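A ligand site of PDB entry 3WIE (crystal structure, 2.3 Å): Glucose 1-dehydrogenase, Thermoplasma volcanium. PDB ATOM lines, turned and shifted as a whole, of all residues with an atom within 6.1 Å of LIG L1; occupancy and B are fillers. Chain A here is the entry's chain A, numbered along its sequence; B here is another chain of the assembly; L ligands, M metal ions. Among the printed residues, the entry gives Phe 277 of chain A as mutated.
The side-chain carboxylate (OE1) of Glu 156 is in hydrogen-bond range of an oxygen (O2) of LIG L1. An oxygen (O4) of LIG L1 sits at hydrogen-bond distance from the side-chain carboxylate (OD2) of Asp 306, at 2.7 Å. ND2 of Asn 160 sits at hydrogen-bond distance from O2 of LIG L1, at 2.8 Å. NZ of Lys 159 sits at hydrogen-bond distance from O3 of LIG L1 (2.9 Å). An oxygen (O4) of LIG L1 sits at hydrogen-bond distance from the side-chain carboxylate of Glu 119. A ring nitrogen (NE2) of His 68 lies within hydrogen-bond range of an oxygen (O1) of LIG L1, at 3.4 Å. The side-chain hydroxyl (OG1) of Thr 43 is in hydrogen-bond range of an oxygen (O6) of LIG L1 (3.4 Å). N of Asp 306 lies within hydrogen-bond range of O18 of LG2 L2, 3.0 Å away. The backbone NH (N) of Phe 277 sits at hydrogen-bond distance from an oxygen (O12) of LG2 L2. O of Phe 277 is in hydrogen-bond range of O12 of LG2 L2 (2.8 Å). The backbone NH of Glu 197 is in hydrogen-bond range of an oxygen (O9) of LG2 L2, 2.8 Å away.
Cys 41 touches LIG L1 (SG to O1, 3.99 Å). NH2 of Arg 94 touches O4 of LIG L1, at 3.7 Å. Phe 277 touches LIG L1 (CZ to O6, 3.6 Å). Val 305 touches LIG L1. Glu 296 of chain B touches LIG L1 (OE2 to C5, 3.9 Å). Hydrophobic or aromatic side chains that line LIG L1: His 68, Phe 277 and Val 305.
The backbone carbonyl oxygen of Glu 156 sits at hydrogen-bond distance from the side-chain amide nitrogen of Asn 160 (3.3 Å). The side-chain carboxylate (OE1) of Glu 156 lies within salt-bridge range of the side-chain amino group (NZ) of Lys 159 (3.3 Å). The side-chain carboxylate of Asp 306 is in salt-bridge range of the side-chain amino group of Lys 159 (3.2 Å). The side-chain carboxylate of Asp 306 is in salt-bridge range of the guanidinium group of Arg 94. The side-chain amino group (NZ) of Lys 159 lies within hydrogen-bond range of the side-chain amide oxygen (OD1) of Asn 160 (2.8 Å). The side-chain amide nitrogen (ND2) of Asn 160 is in hydrogen-bond range of the side-chain carboxylate (OE1) of Glu 197, at 3.5 Å. The side-chain carboxylate (OE1) of Glu 119 lies within salt-bridge range of the guanidinium group (NH2) of Arg 94 (2.7 Å). The side-chain sulfur (SG) of Cys 41 lies close to the backbone NH (N) of Thr 43.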
ATOM      1  N   CYS A  41     -12.592 -14.771  24.619  1.00  0.00           N
ATOM      2  CA  CYS A  41     -13.768 -14.883  23.752  1.00  0.00           C
ATOM      3  C   CYS A  41     -13.838 -16.358  23.384  1.00  0.00           C
ATOM      4  O   CYS A  41     -12.931 -17.141  23.709  1.00  0.00           O
ATOM      5  CB  CYS A  41     -13.653 -13.978  22.485  1.00  0.00           C
ATOM      6  SG  CYS A  41     -12.624 -14.717  21.172  1.00  0.00           S
ATOM      7  N   THR A  43     -13.454 -18.069  20.770  1.00  0.00           N
ATOM      8  CA  THR A  43     -12.339 -18.570  20.007  1.00  0.00           C
ATOM      9  C   THR A  43     -11.210 -19.069  20.957  1.00  0.00           C
ATOM     10  O   THR A  43     -10.712 -20.184  20.816  1.00  0.00           O
ATOM     11  CB  THR A  43     -11.800 -17.446  19.053  1.00  0.00           C
ATOM     12  OG1 THR A  43     -12.787 -17.108  18.050  1.00  0.00           O
ATOM     13  CG2 THR A  43     -10.513 -17.870  18.397  1.00  0.00           C
ATOM     14  N   PHE A  54      -8.388 -25.453  12.258  1.00  0.00           N
ATOM     15  CA  PHE A  54      -7.631 -24.480  11.445  1.00  0.00           C
ATOM     16  C   PHE A  54      -6.488 -23.752  12.232  1.00  0.00           C
ATOM     17  O   PHE A  54      -5.620 -23.128  11.636  1.00  0.00           O
ATOM     18  CB  PHE A  54      -8.563 -23.454  10.751  1.00  0.00           C
ATOM     19  CG  PHE A  54      -9.336 -22.555  11.691  1.00  0.00           C
ATOM     20  CD1 PHE A  54     -10.529 -22.988  12.287  1.00  0.00           C
ATOM     21  CD2 PHE A  54      -8.901 -21.260  11.966  1.00  0.00           C
ATOM     22  CE1 PHE A  54     -11.243 -22.152  13.140  1.00  0.00           C
ATOM     23  CE2 PHE A  54      -9.605 -20.419  12.806  1.00  0.00           C
ATOM     24  CZ  PHE A  54     -10.786 -20.869  13.388  1.00  0.00           C
ATOM     25  N   HIS A  68      -5.664 -12.590  21.807  1.00  0.00           N
ATOM     26  CA  HIS A  68      -5.743 -11.681  20.694  1.00  0.00           C
ATOM     27  C   HIS A  68      -6.464 -10.399  20.980  1.00  0.00           C
ATOM     28  O   HIS A  68      -6.331  -9.436  20.217  1.00  0.00           O
ATOM     29  CB  HIS A  68      -6.277 -12.407  19.485  1.00  0.00           C
ATOM     30  CG  HIS A  68      -7.642 -12.963  19.656  1.00  0.00           C
ATOM     31  ND1 HIS A  68      -7.881 -14.135  20.330  1.00  0.00           N
ATOM     32  CD2 HIS A  68      -8.840 -12.521  19.207  1.00  0.00           C
ATOM     33  CE1 HIS A  68      -9.169 -14.394  20.315  1.00  0.00           C
ATOM     34  NE2 HIS A  68      -9.770 -13.441  19.627  1.00  0.00           N
ATOM     35  N   GLU A  69      -7.172 -10.307  22.104  1.00  0.00           N
ATOM     36  CA  GLU A  69      -7.881  -9.049  22.427  1.00  0.00           C
ATOM     37  C   GLU A  69      -7.064  -8.312  23.491  1.00  0.00           C
ATOM     38  O   GLU A  69      -7.156  -8.649  24.663  1.00  0.00           O
ATOM     39  CB  GLU A  69      -9.304  -9.318  22.952  1.00  0.00           C
ATOM     40  CG  GLU A  69      -9.988 -10.531  22.332  1.00  0.00           C
ATOM     41  CD  GLU A  69     -11.435 -10.767  22.860  1.00  0.00           C
ATOM     42  OE1 GLU A  69     -11.911 -10.076  23.797  1.00  0.00           O
ATOM     43  OE2 GLU A  69     -12.095 -11.686  22.335  1.00  0.00           O
ATOM     44  N   VAL A  93      -4.649  -7.936  15.277  1.00  0.00           N
ATOM     45  CA  VAL A  93      -4.627  -9.373  15.361  1.00  0.00           C
ATOM     46  C   VAL A  93      -4.117  -9.989  14.047  1.00  0.00           C
ATOM     47  O   VAL A  93      -3.254 -10.877  14.061  1.00  0.00           O
ATOM     48  CB  VAL A  93      -6.018  -9.979  15.614  1.00  0.00           C
ATOM     49  CG1 VAL A  93      -5.909 -11.473  15.701  1.00  0.00           C
ATOM     50  CG2 VAL A  93      -6.660  -9.438  16.879  1.00  0.00           C
ATOM     51  N   ARG A  94      -4.731  -9.564  12.935  1.00  0.00           N
ATOM     52  CA  ARG A  94      -4.447 -10.136  11.626  1.00  0.00           C
ATOM     53  C   ARG A  94      -3.384  -9.375  10.926  1.00  0.00           C
ATOM     54  O   ARG A  94      -3.482  -8.129  10.779  1.00  0.00           O
ATOM     55  CB  ARG A  94      -5.646 -10.144  10.724  1.00  0.00           C
ATOM     56  CG  ARG A  94      -5.435 -11.040   9.548  1.00  0.00           C
ATOM     57  CD  ARG A  94      -6.627 -11.103   8.608  1.00  0.00           C
ATOM     58  NE  ARG A  94      -7.595 -12.049   9.073  1.00  0.00           N
ATOM     59  CZ  ARG A  94      -8.527 -12.616   8.306  1.00  0.00           C
ATOM     60  NH1 ARG A  94      -8.627 -12.341   6.995  1.00  0.00           N
ATOM     61  NH2 ARG A  94      -9.378 -13.455   8.859  1.00  0.00           N
ATOM     62  N   GLU A 119      -2.911 -14.726  12.126  1.00  0.00           N
ATOM     63  CA  GLU A 119      -3.603 -14.096  13.250  1.00  0.00           C
ATOM     64  C   GLU A 119      -2.917 -14.386  14.555  1.00  0.00           C
ATOM     65  O   GLU A 119      -2.611 -15.533  14.904  1.00  0.00           O
ATOM     66  CB  GLU A 119      -5.039 -14.563  13.368  1.00  0.00           C
ATOM     67  CG  GLU A 119      -5.995 -13.901  12.366  1.00  0.00           C
ATOM     68  CD  GLU A 119      -6.683 -14.881  11.418  1.00  0.00           C
ATOM     69  OE1 GLU A 119      -7.585 -14.443  10.687  1.00  0.00           O
ATOM     70  OE2 GLU A 119      -6.348 -16.071  11.406  1.00  0.00           O
ATOM     71  N   ILE A 122      -3.833 -17.356  17.099  1.00  0.00           N
ATOM     72  CA  ILE A 122      -4.723 -18.271  16.441  1.00  0.00           C
ATOM     73  C   ILE A 122      -4.041 -19.076  15.354  1.00  0.00           C
ATOM     74  O   ILE A 122      -4.089 -20.263  15.345  1.00  0.00           O
ATOM     75  CB  ILE A 122      -5.878 -17.499  15.831  1.00  0.00           C
ATOM     76  CG1 ILE A 122      -6.542 -16.682  16.914  1.00  0.00           C
ATOM     77  CG2 ILE A 122      -6.898 -18.432  15.230  1.00  0.00           C
ATOM     78  CD1 ILE A 122      -7.412 -15.604  16.390  1.00  0.00           C
ATOM     79  N   GLU A 156     -10.803  -4.776  20.324  1.00  0.00           N
ATOM     80  CA  GLU A 156     -10.702  -5.868  19.380  1.00  0.00           C
ATOM     81  C   GLU A 156     -12.059  -6.532  19.053  1.00  0.00           C
ATOM     82  O   GLU A 156     -12.402  -6.757  17.865  1.00  0.00           O
ATOM     83  CB  GLU A 156      -9.679  -6.871  19.864  1.00  0.00           C
ATOM     84  CG  GLU A 156      -9.178  -7.846  18.819  1.00  0.00           C
ATOM     85  CD  GLU A 156     -10.204  -8.916  18.495  1.00  0.00           C
ATOM     86  OE1 GLU A 156      -9.939  -9.792  17.641  1.00  0.00           O
ATOM     87  OE2 GLU A 156     -11.285  -8.849  19.060  1.00  0.00           O
ATOM     88  N   PRO A 157     -12.845  -6.858  20.076  1.00  0.00           N
ATOM     89  CA  PRO A 157     -14.163  -7.343  19.692  1.00  0.00           C
ATOM     90  C   PRO A 157     -15.000  -6.271  18.958  1.00  0.00           C
ATOM     91  O   PRO A 157     -15.756  -6.609  18.048  1.00  0.00           O
ATOM     92  CB  PRO A 157     -14.777  -7.789  21.007  1.00  0.00           C
ATOM     93  CG  PRO A 157     -13.998  -7.074  22.080  1.00  0.00           C
ATOM     94  CD  PRO A 157     -12.616  -6.878  21.534  1.00  0.00           C
ATOM     95  N   LYS A 159     -13.927  -3.802  16.850  1.00  0.00           N
ATOM     96  CA  LYS A 159     -13.463  -3.529  15.480  1.00  0.00           C
ATOM     97  C   LYS A 159     -14.112  -4.491  14.513  1.00  0.00           C
ATOM     98  O   LYS A 159     -14.389  -4.106  13.403  1.00  0.00           O
ATOM     99  CB  LYS A 159     -11.948  -3.460  15.306  1.00  0.00           C
ATOM    100  CG  LYS A 159     -11.133  -4.655  15.753  1.00  0.00           C
ATOM    101  CD  LYS A 159     -11.102  -5.837  14.828  1.00  0.00           C
ATOM    102  CE  LYS A 159     -10.380  -6.955  15.522  1.00  0.00           C
ATOM    103  NZ  LYS A 159     -10.339  -8.242  14.801  1.00  0.00           N
ATOM    104  N   ASN A 160     -14.423  -5.710  14.945  1.00  0.00           N
ATOM    105  CA  ASN A 160     -15.159  -6.634  14.111  1.00  0.00           C
ATOM    106  C   ASN A 160     -16.567  -6.120  13.756  1.00  0.00           C
ATOM    107  O   ASN A 160     -17.059  -6.293  12.631  1.00  0.00           O
ATOM    108  CB  ASN A 160     -15.278  -7.958  14.794  1.00  0.00           C
ATOM    109  CG  ASN A 160     -13.929  -8.637  14.983  1.00  0.00           C
ATOM    110  OD1 ASN A 160     -13.078  -8.610  14.113  1.00  0.00           O
ATOM    111  ND2 ASN A 160     -13.714  -9.263  16.149  1.00  0.00           N
ATOM    112  N   GLU A 197     -20.369  -9.604  21.885  1.00  0.00           N
ATOM    113  CA  GLU A 197     -20.400  -9.066  20.519  1.00  0.00           C
ATOM    114  C   GLU A 197     -21.813  -8.515  20.212  1.00  0.00           C
ATOM    115  O   GLU A 197     -21.949  -7.426  19.634  1.00  0.00           O
ATOM    116  CB  GLU A 197     -19.914 -10.087  19.475  1.00  0.00           C
ATOM    117  CG  GLU A 197     -18.402 -10.431  19.532  1.00  0.00           C
ATOM    118  CD  GLU A 197     -17.505  -9.379  18.835  1.00  0.00           C
ATOM    119  OE1 GLU A 197     -16.481  -9.716  18.205  1.00  0.00           O
ATOM    120  OE2 GLU A 197     -17.841  -8.183  18.900  1.00  0.00           O
ATOM    121  N   PHE A 277     -19.879 -18.077  14.702  1.00  0.00           N
ATOM    122  CA  PHE A 277     -19.615 -19.381  14.155  1.00  0.00           C
ATOM    123  C   PHE A 277     -19.409 -20.434  15.229  1.00  0.00           C
ATOM    124  O   PHE A 277     -18.823 -20.202  16.273  1.00  0.00           O
ATOM    125  CB  PHE A 277     -18.478 -19.369  13.132  1.00  0.00           C
ATOM    126  CG  PHE A 277     -17.106 -19.021  13.673  1.00  0.00           C
ATOM    127  CD1 PHE A 277     -16.310 -19.989  14.270  1.00  0.00           C
ATOM    128  CD2 PHE A 277     -16.583 -17.742  13.498  1.00  0.00           C
ATOM    129  CE1 PHE A 277     -15.032 -19.678  14.722  1.00  0.00           C
ATOM    130  CE2 PHE A 277     -15.307 -17.422  13.944  1.00  0.00           C
ATOM    131  CZ  PHE A 277     -14.532 -18.384  14.558  1.00  0.00           C
ATOM    132  N   VAL A 305     -15.773 -11.352   8.595  1.00  0.00           N
ATOM    133  CA  VAL A 305     -14.773 -11.713   9.576  1.00  0.00           C
ATOM    134  C   VAL A 305     -13.667 -10.695   9.616  1.00  0.00           C
ATOM    135  O   VAL A 305     -13.243 -10.200   8.602  1.00  0.00           O
ATOM    136  CB  VAL A 305     -14.201 -13.093   9.330  1.00  0.00           C
ATOM    137  CG1 VAL A 305     -13.390 -13.109   8.071  1.00  0.00           C
ATOM    138  CG2 VAL A 305     -13.355 -13.525  10.486  1.00  0.00           C
ATOM    139  N   ASP A 306     -13.224 -10.377  10.830  1.00  0.00           N
ATOM    140  CA  ASP A 306     -12.059  -9.539  11.118  1.00  0.00           C
ATOM    141  C   ASP A 306     -12.282  -8.083  10.793  1.00  0.00           C
ATOM    142  O   ASP A 306     -13.372  -7.704  10.522  1.00  0.00           O
ATOM    143  CB  ASP A 306     -10.797 -10.094  10.497  1.00  0.00           C
ATOM    144  CG  ASP A 306      -9.630  -9.990  11.414  1.00  0.00           C
ATOM    145  OD1 ASP A 306      -9.343  -8.902  11.866  1.00  0.00           O
ATOM    146  OD2 ASP A 306      -9.018 -10.998  11.723  1.00  0.00           O
ATOM    147  N   ALA A 307     -11.252  -7.265  10.820  1.00  0.00           N
ATOM    148  CA  ALA A 307     -11.387  -5.868  10.454  1.00  0.00           C
ATOM    149  C   ALA A 307     -10.066  -5.260  10.070  1.00  0.00           C
ATOM    150  O   ALA A 307      -9.060  -5.780  10.353  1.00  0.00           O
ATOM    151  CB  ALA A 307     -12.044  -5.103  11.565  1.00  0.00           C
ATOM    152  N   TYR A 312     -10.130  -0.475  14.036  1.00  0.00           N
ATOM    153  CA  TYR A 312      -9.629  -0.308  15.380  1.00  0.00           C
ATOM    154  C   TYR A 312      -9.669   1.154  15.769  1.00  0.00           C
ATOM    155  O   TYR A 312     -10.045   1.506  16.882  1.00  0.00           O
ATOM    156  CB  TYR A 312      -8.182  -0.797  15.521  1.00  0.00           C
ATOM    157  CG  TYR A 312      -7.922  -2.274  15.395  1.00  0.00           C
ATOM    158  CD1 TYR A 312      -8.123  -2.924  14.193  1.00  0.00           C
ATOM    159  CD2 TYR A 312      -7.458  -3.038  16.482  1.00  0.00           C
ATOM    160  CE1 TYR A 312      -7.878  -4.278  14.023  1.00  0.00           C
ATOM    161  CE2 TYR A 312      -7.157  -4.431  16.314  1.00  0.00           C
ATOM    162  CZ  TYR A 312      -7.353  -5.045  15.071  1.00  0.00           C
ATOM    163  OH  TYR A 312      -7.074  -6.416  14.822  1.00  0.00           O
ATOM    164  N   GLU B 296     -15.992 -17.044   7.473  1.00  0.00           N
ATOM    165  CA  GLU B 296     -14.540 -16.967   7.370  1.00  0.00           C
ATOM    166  C   GLU B 296     -14.068 -16.499   5.998  1.00  0.00           C
ATOM    167  O   GLU B 296     -13.004 -15.964   5.895  1.00  0.00           O
ATOM    168  CB  GLU B 296     -13.840 -18.291   7.751  1.00  0.00           C
ATOM    169  CG  GLU B 296     -13.909 -18.594   9.257  1.00  0.00           C
ATOM    170  CD  GLU B 296     -12.542 -18.794   9.885  1.00  0.00           C
ATOM    171  OE1 GLU B 296     -11.900 -19.822   9.537  1.00  0.00           O
ATOM    172  OE2 GLU B 296     -12.098 -17.950  10.718  1.00  0.00           O
HETATM  173  C1  LIG L   1     -11.131 -12.296  15.967  1.00  0.00           C
HETATM  174  C2  LIG L   1     -10.809 -12.080  14.480  1.00  0.00           C
HETATM  175  C3  LIG L   1     -10.340 -13.408  13.825  1.00  0.00           C
HETATM  176  C4  LIG L   1     -11.401 -14.403  14.070  1.00  0.00           C
HETATM  177  C5  LIG L   1     -10.947 -15.811  13.820  1.00  0.00           C
HETATM  178  C6  LIG L   1     -12.122 -13.355  16.036  1.00  0.00           C
HETATM  179  O1  LIG L   1     -12.230 -13.732  17.329  1.00  0.00           O
HETATM  180  O2  LIG L   1     -11.672 -11.188  16.484  1.00  0.00           O
HETATM  181  O3  LIG L   1      -9.850 -11.085  14.363  1.00  0.00           O
HETATM  182  O4  LIG L   1     -10.200 -13.283  12.441  1.00  0.00           O
HETATM  183  O5  LIG L   1     -11.555 -14.498  15.449  1.00  0.00           O
HETATM  184  O6  LIG L   1     -11.409 -16.586  14.936  1.00  0.00           O
HETATM  185  P1  LG2 L   2     -20.480 -15.233  23.247  1.00  0.00           P
HETATM  186  O1  LG2 L   2     -20.503 -14.301  24.384  1.00  0.00           O
HETATM  187  O2  LG2 L   2     -20.414 -16.707  23.400  1.00  0.00           O
HETATM  188  O3  LG2 L   2     -21.891 -14.910  22.516  1.00  0.00           O
HETATM  189  C1  LG2 L   2     -22.713 -15.893  21.866  1.00  0.00           C
HETATM  190  C2  LG2 L   2     -24.158 -15.457  22.071  1.00  0.00           C
HETATM  191  O4  LG2 L   2     -24.974 -16.304  21.269  1.00  0.00           O
HETATM  192  C3  LG2 L   2     -24.570 -15.671  23.539  1.00  0.00           C
HETATM  193  O5  LG2 L   2     -25.472 -14.654  23.964  1.00  0.00           O
HETATM  194  C4  LG2 L   2     -25.256 -16.991  23.463  1.00  0.00           C
HETATM  195  O6  LG2 L   2     -26.149 -17.115  24.587  1.00  0.00           O
HETATM  196  C5  LG2 L   2     -26.005 -16.767  22.154  1.00  0.00           C
HETATM  197  N1  LG2 L   2     -26.549 -17.968  21.549  1.00  0.00           N
HETATM  198  C6  LG2 L   2     -26.056 -19.202  21.379  1.00  0.00           C
HETATM  199  N2  LG2 L   2     -26.999 -19.937  20.769  1.00  0.00           N
HETATM  200  C7  LG2 L   2     -28.069 -19.144  20.563  1.00  0.00           C
HETATM  201  C8  LG2 L   2     -29.225 -19.368  19.972  1.00  0.00           C
HETATM  202  N3  LG2 L   2     -29.446 -20.584  19.501  1.00  0.00           N
HETATM  203  N4  LG2 L   2     -30.162 -18.442  19.898  1.00  0.00           N
HETATM  204  C9  LG2 L   2     -29.857 -17.170  20.391  1.00  0.00           C
HETATM  205  N5  LG2 L   2     -28.634 -16.919  20.995  1.00  0.00           N
HETATM  206  C10 LG2 L   2     -27.778 -17.927  21.062  1.00  0.00           C
HETATM  207  O7  LG2 L   2     -19.237 -14.765  22.262  1.00  0.00           O
HETATM  208  P2  LG2 L   2     -19.076 -13.273  21.435  1.00  0.00           P
HETATM  209  O8  LG2 L   2     -17.670 -12.752  21.614  1.00  0.00           O
HETATM  210  O9  LG2 L   2     -20.224 -12.391  21.812  1.00  0.00           O
HETATM  211  O10 LG2 L   2     -19.246 -13.825  19.900  1.00  0.00           O
HETATM  212  C11 LG2 L   2     -20.072 -14.966  19.571  1.00  0.00           C
HETATM  213  C12 LG2 L   2     -19.615 -15.464  18.213  1.00  0.00           C
HETATM  214  O11 LG2 L   2     -18.873 -14.459  17.462  1.00  0.00           O
HETATM  215  C13 LG2 L   2     -18.677 -16.659  18.339  1.00  0.00           C
HETATM  216  O12 LG2 L   2     -19.169 -17.685  17.497  1.00  0.00           O
HETATM  217  C14 LG2 L   2     -17.341 -16.163  17.789  1.00  0.00           C
HETATM  218  O13 LG2 L   2     -16.651 -17.147  17.046  1.00  0.00           O
HETATM  219  C15 LG2 L   2     -17.822 -15.182  16.789  1.00  0.00           C
HETATM  220  N6  LG2 L   2     -16.819 -14.190  16.381  1.00  0.00           N
HETATM  221  C16 LG2 L   2     -16.766 -13.853  15.026  1.00  0.00           C
HETATM  222  C17 LG2 L   2     -15.879 -12.895  14.560  1.00  0.00           C
HETATM  223  C18 LG2 L   2     -15.797 -12.546  13.200  1.00  0.00           C
HETATM  224  O14 LG2 L   2     -16.512 -13.136  12.303  1.00  0.00           O
HETATM  225  C19 LG2 L   2     -15.060 -12.246  15.501  1.00  0.00           C
HETATM  226  C20 LG2 L   2     -15.127 -12.557  16.865  1.00  0.00           C
HETATM  227  C21 LG2 L   2     -16.001 -13.532  17.318  1.00  0.00           C
HETATM  228  P3  LG2 L   2     -25.789 -18.116  25.872  1.00  0.00           P
HETATM  229  O15 LG2 L   2     -24.540 -17.668  26.498  1.00  0.00           O
HETATM  230  O16 LG2 L   2     -27.116 -17.884  26.774  1.00  0.00           O
HETATM  231  O17 LG2 L   2     -25.721 -19.631  25.230  1.00  0.00           O
HETATM  232  O18 LG2 L   2     -15.002 -11.598  12.925  1.00  0.00           O
HETATM  233 ZN    ZN M   1     -12.357 -12.693  20.422  1.00  0.00          ZN
